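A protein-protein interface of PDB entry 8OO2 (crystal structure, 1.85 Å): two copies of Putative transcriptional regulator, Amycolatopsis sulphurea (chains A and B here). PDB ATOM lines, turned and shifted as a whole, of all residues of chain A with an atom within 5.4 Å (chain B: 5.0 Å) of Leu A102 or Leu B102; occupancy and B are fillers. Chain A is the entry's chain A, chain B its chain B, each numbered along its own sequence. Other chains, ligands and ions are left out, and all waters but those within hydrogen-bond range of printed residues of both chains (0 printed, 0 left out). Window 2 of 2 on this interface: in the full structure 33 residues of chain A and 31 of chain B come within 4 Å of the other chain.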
ATOM      1  N   LEU A  25       0.426  25.379 -27.986  1.00  0.00           N
ATOM      2  CA  LEU A  25       0.273  24.660 -29.258  1.00  0.00           C
ATOM      3  C   LEU A  25      -0.991  23.827 -29.258  1.00  0.00           C
ATOM      4  O   LEU A  25      -1.618  23.638 -30.300  1.00  0.00           O
ATOM      5  CB  LEU A  25       1.495  23.797 -29.513  1.00  0.00           C
ATOM      6  CG  LEU A  25       1.491  22.964 -30.784  1.00  0.00           C
ATOM      7  CD1 LEU A  25       1.360  23.818 -31.989  1.00  0.00           C
ATOM      8  CD2 LEU A  25       2.774  22.106 -30.847  1.00  0.00           C
ATOM      9  N   ASP A  99       5.428  27.753 -26.289  1.00  0.00           N
ATOM     10  CA  ASP A  99       5.578  26.527 -27.060  1.00  0.00           C
ATOM     11  C   ASP A  99       6.284  26.785 -28.412  1.00  0.00           C
ATOM     12  O   ASP A  99       5.943  26.139 -29.386  1.00  0.00           O
ATOM     13  CB  ASP A  99       4.251  25.873 -27.320  1.00  0.00           C
ATOM     14  CG  ASP A  99       3.620  25.273 -26.013  1.00  0.00           C
ATOM     15  OD1 ASP A  99       2.452  25.044 -25.983  1.00  0.00           O
ATOM     16  OD2 ASP A  99       4.414  25.068 -25.057  1.00  0.00           O
ATOM     17  N   GLY A 100       7.192  27.754 -28.454  1.00  0.00           N
ATOM     18  CA  GLY A 100       7.813  28.135 -29.719  1.00  0.00           C
ATOM     19  C   GLY A 100       8.583  26.986 -30.355  1.00  0.00           C
ATOM     20  O   GLY A 100       8.407  26.722 -31.538  1.00  0.00           O
ATOM     21  N   ALA A 101       9.401  26.302 -29.566  1.00  0.00           N
ATOM     22  CA  ALA A 101      10.194  25.171 -30.109  1.00  0.00           C
ATOM     23  C   ALA A 101       9.294  24.013 -30.491  1.00  0.00           C
ATOM     24  O   ALA A 101       9.540  23.333 -31.494  1.00  0.00           O
ATOM     25  CB  ALA A 101      11.228  24.742 -29.091  1.00  0.00           C
ATOM     26  N   LEU A 102       8.221  23.756 -29.710  1.00  0.00           N
ATOM     27  CA  LEU A 102       7.313  22.685 -30.073  1.00  0.00           C
ATOM     28  C   LEU A 102       6.585  22.994 -31.373  1.00  0.00           C
ATOM     29  O   LEU A 102       6.285  22.086 -32.147  1.00  0.00           O
ATOM     30  CB  LEU A 102       6.299  22.452 -28.929  1.00  0.00           C
ATOM     31  CG  LEU A 102       6.813  21.799 -27.656  1.00  0.00           C
ATOM     32  CD1 LEU A 102       5.644  21.653 -26.643  1.00  0.00           C
ATOM     33  CD2 LEU A 102       7.414  20.434 -27.940  1.00  0.00           C
ATOM     34  N   LEU A 103       6.197  24.242 -31.586  1.00  0.00           N
ATOM     35  CA  LEU A 103       5.538  24.642 -32.849  1.00  0.00           C
ATOM     36  C   LEU A 103       6.525  24.381 -33.982  1.00  0.00           C
ATOM     37  O   LEU A 103       6.145  23.830 -34.994  1.00  0.00           O
ATOM     38  CB  LEU A 103       5.179  26.125 -32.766  1.00  0.00           C
ATOM     39  CG  LEU A 103       4.596  26.777 -34.019  1.00  0.00           C
ATOM     40  CD1 LEU A 103       5.678  27.137 -35.023  1.00  0.00           C
ATOM     41  CD2 LEU A 103       3.540  25.900 -34.660  1.00  0.00           C
ATOM     42  N   HIS A 104       7.767  24.763 -33.763  1.00  0.00           N
ATOM     43  CA  HIS A 104       8.806  24.663 -34.804  1.00  0.00           C
ATOM     44  C   HIS A 104       9.161  23.206 -35.093  1.00  0.00           C
ATOM     45  O   HIS A 104       9.363  22.895 -36.202  1.00  0.00           O
ATOM     46  CB  HIS A 104      10.023  25.443 -34.340  1.00  0.00           C
ATOM     47  CG  HIS A 104      10.995  25.722 -35.411  1.00  0.00           C
ATOM     48  ND1 HIS A 104      10.802  26.691 -36.366  1.00  0.00           N
ATOM     49  CD2 HIS A 104      12.160  25.162 -35.675  1.00  0.00           C
ATOM     50  CE1 HIS A 104      11.840  26.712 -37.170  1.00  0.00           C
ATOM     51  NE2 HIS A 104      12.668  25.793 -36.765  1.00  0.00           N
ATOM     52  N   ALA A 105       9.282  22.355 -34.103  1.00  0.00           N
ATOM     53  CA  ALA A 105       9.739  20.972 -34.325  1.00  0.00           C
ATOM     54  C   ALA A 105       8.970  20.346 -35.484  1.00  0.00           C
ATOM     55  O   ALA A 105       7.748  20.366 -35.438  1.00  0.00           O
ATOM     56  CB  ALA A 105       9.580  20.165 -33.067  1.00  0.00           C
ATOM     57  N   ILE A 150      14.558  23.567 -26.825  1.00  0.00           N
ATOM     58  CA  ILE A 150      13.514  22.641 -26.336  1.00  0.00           C
ATOM     59  C   ILE A 150      13.944  22.000 -25.054  1.00  0.00           C
ATOM     60  O   ILE A 150      13.098  21.678 -24.191  1.00  0.00           O
ATOM     61  CB  ILE A 150      13.173  21.642 -27.438  1.00  0.00           C
ATOM     62  CG1 ILE A 150      11.784  21.018 -27.182  1.00  0.00           C
ATOM     63  CG2 ILE A 150      14.216  20.526 -27.509  1.00  0.00           C
ATOM     64  CD1 ILE A 150      10.973  20.841 -28.436  1.00  0.00           C
ATOM     65  N   LEU B  25       3.100  10.465 -24.669  1.00  0.00           N
ATOM     66  CA  LEU B  25       3.410  11.374 -23.570  1.00  0.00           C
ATOM     67  C   LEU B  25       2.139  11.991 -23.000  1.00  0.00           C
ATOM     68  O   LEU B  25       2.086  12.278 -21.798  1.00  0.00           O
ATOM     69  CB  LEU B  25       4.371  12.462 -24.038  1.00  0.00           C
ATOM     70  CG  LEU B  25       4.839  13.466 -22.986  1.00  0.00           C
ATOM     71  CD1 LEU B  25       5.463  12.769 -21.798  1.00  0.00           C
ATOM     72  CD2 LEU B  25       5.816  14.452 -23.596  1.00  0.00           C
ATOM     73  N   ASP B  99       7.108   9.239 -28.803  1.00  0.00           N
ATOM     74  CA  ASP B  99       7.324  10.520 -28.148  1.00  0.00           C
ATOM     75  C   ASP B  99       8.613  10.516 -27.327  1.00  0.00           C
ATOM     76  O   ASP B  99       8.696  11.183 -26.289  1.00  0.00           O
ATOM     77  CB  ASP B  99       6.134  10.892 -27.246  1.00  0.00           C
ATOM     78  CG  ASP B  99       4.865  11.178 -28.053  1.00  0.00           C
ATOM     79  OD1 ASP B  99       4.985  11.524 -29.248  1.00  0.00           O
ATOM     80  OD2 ASP B  99       3.768  11.032 -27.494  1.00  0.00           O
ATOM     81  N   GLY B 100       9.622   9.796 -27.804  1.00  0.00           N
ATOM     82  CA  GLY B 100      10.859   9.678 -27.071  1.00  0.00           C
ATOM     83  C   GLY B 100      11.537  11.008 -26.841  1.00  0.00           C
ATOM     84  O   GLY B 100      11.924  11.318 -25.707  1.00  0.00           O
ATOM     85  N   ALA B 101      11.726  11.780 -27.913  1.00  0.00           N
ATOM     86  CA  ALA B 101      12.360  13.086 -27.802  1.00  0.00           C
ATOM     87  C   ALA B 101      11.495  14.054 -27.001  1.00  0.00           C
ATOM     88  O   ALA B 101      12.018  14.864 -26.221  1.00  0.00           O
ATOM     89  CB  ALA B 101      12.602  13.665 -29.196  1.00  0.00           C
ATOM     90  N   LEU B 102      10.177  13.983 -27.157  1.00  0.00           N
ATOM     91  CA  LEU B 102       9.292  14.829 -26.354  1.00  0.00           C
ATOM     92  C   LEU B 102       9.400  14.503 -24.876  1.00  0.00           C
ATOM     93  O   LEU B 102       9.376  15.421 -24.015  1.00  0.00           O
ATOM     94  CB  LEU B 102       7.851  14.666 -26.827  1.00  0.00           C
ATOM     95  CG  LEU B 102       7.516  15.340 -28.174  1.00  0.00           C
ATOM     96  CD1 LEU B 102       6.126  14.904 -28.650  1.00  0.00           C
ATOM     97  CD2 LEU B 102       7.592  16.864 -28.059  1.00  0.00           C
ATOM     98  N   LEU B 103       9.489  13.201 -24.547  1.00  0.00           N
ATOM     99  CA  LEU B 103       9.674  12.808 -23.153  1.00  0.00           C
ATOM    100  C   LEU B 103      11.011  13.319 -22.628  1.00  0.00           C
ATOM    101  O   LEU B 103      11.121  13.794 -21.497  1.00  0.00           O
ATOM    102  CB  LEU B 103       9.590  11.277 -23.041  1.00  0.00           C
ATOM    103  CG  LEU B 103       9.864  10.572 -21.719  1.00  0.00           C
ATOM    104  CD1 LEU B 103      11.327  10.601 -21.340  1.00  0.00           C
ATOM    105  CD2 LEU B 103       9.034  11.141 -20.611  1.00  0.00           C
ATOM    106  N   HIS B 104      12.055  13.243 -23.456  1.00  0.00           N
ATOM    107  CA  HIS B 104      13.370  13.614 -22.951  1.00  0.00           C
ATOM    108  C   HIS B 104      13.486  15.123 -22.732  1.00  0.00           C
ATOM    109  O   HIS B 104      14.146  15.579 -21.778  1.00  0.00           O
ATOM    110  CB  HIS B 104      14.455  13.200 -23.927  1.00  0.00           C
ATOM    111  CG  HIS B 104      15.836  13.374 -23.384  1.00  0.00           C
ATOM    112  ND1 HIS B 104      16.532  12.383 -22.711  1.00  0.00           N
ATOM    113  CD2 HIS B 104      16.613  14.455 -23.357  1.00  0.00           C
ATOM    114  CE1 HIS B 104      17.695  12.866 -22.305  1.00  0.00           C
ATOM    115  NE2 HIS B 104      17.755  14.137 -22.667  1.00  0.00           N
ATOM    116  N   ALA B 105      12.873  15.887 -23.589  1.00  0.00           N
ATOM    117  CA  ALA B 105      13.110  17.330 -23.632  1.00  0.00           C
ATOM    118  C   ALA B 105      12.802  17.931 -22.266  1.00  0.00           C
ATOM    119  O   ALA B 105      11.729  17.718 -21.686  1.00  0.00           O
ATOM    120  CB  ALA B 105      12.241  17.965 -24.716  1.00  0.00           C
ATOM    121  N   ILE B 150      13.999  15.470 -32.758  1.00  0.00           N
ATOM    122  CA  ILE B 150      12.673  16.067 -32.632  1.00  0.00           C
ATOM    123  C   ILE B 150      12.263  16.777 -33.908  1.00  0.00           C
ATOM    124  O   ILE B 150      11.057  16.893 -34.191  1.00  0.00           O
ATOM    125  CB  ILE B 150      12.646  17.014 -31.417  1.00  0.00           C
ATOM    126  CG1 ILE B 150      11.191  17.246 -30.965  1.00  0.00           C
ATOM    127  CG2 ILE B 150      13.297  18.314 -31.747  1.00  0.00           C
ATOM    128  CD1 ILE B 150      11.061  17.351 -29.467  1.00  0.00           C
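Among the printed residues, pairs that only touch across the chains: Leu A102 with Leu B102 (3.6 Å), Ala A105 with Ile B150 (3.8 Å), Ile A150 with Ala B105 (3.8 Å) and Ile A150 with Ile B150 (3.6 Å).
Ala A101 touches none of the printed residues of chain B. Leu A102 touches just one residue of chain B: Leu B102 (3.6 Å). Printed residues of chain B within 4 Å of Ala A105: Ile B150 (3.8 Å). Leu B25 touches none of the printed residues of chain A. Of chain A, only Leu A102 comes within 4 Å of Leu B102. Of the printed residues of chain A, Ala B105 touches Ile A150. The nearest printed residue of chain B that does not touch Leu A102 is Ile B150 (5.0 Å). The nearest residue of chain A that does not touch Leu B102 is Ile A150 (5.2 Å).
Hydrophobic or aromatic side chains of chain B within 4 Å of the printed part of chain A: Leu B102, Ala B105 and Ile B150. Among the printed residues, 4 pairs touch across the chains. Among the printed residues, no Asp or Glu carboxylate lies within 4 Å of a Lys or Arg side-chain nitrogen of the other chain.
Leu A102 touches its own counterpart, Leu B102. Ala A105 touches Ile B150, and with the chains exchanged Ile A150 touches Ala B105. Ile A150 touches its own counterpart, Ile B150. Positions printed for both chains: 25, 99, 100, 101, 102, 103, 104, 105 and 150. Of the 4 pairs that touch across the chains among the printed residues, 4 have their exchanged pair printed and touching as well.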
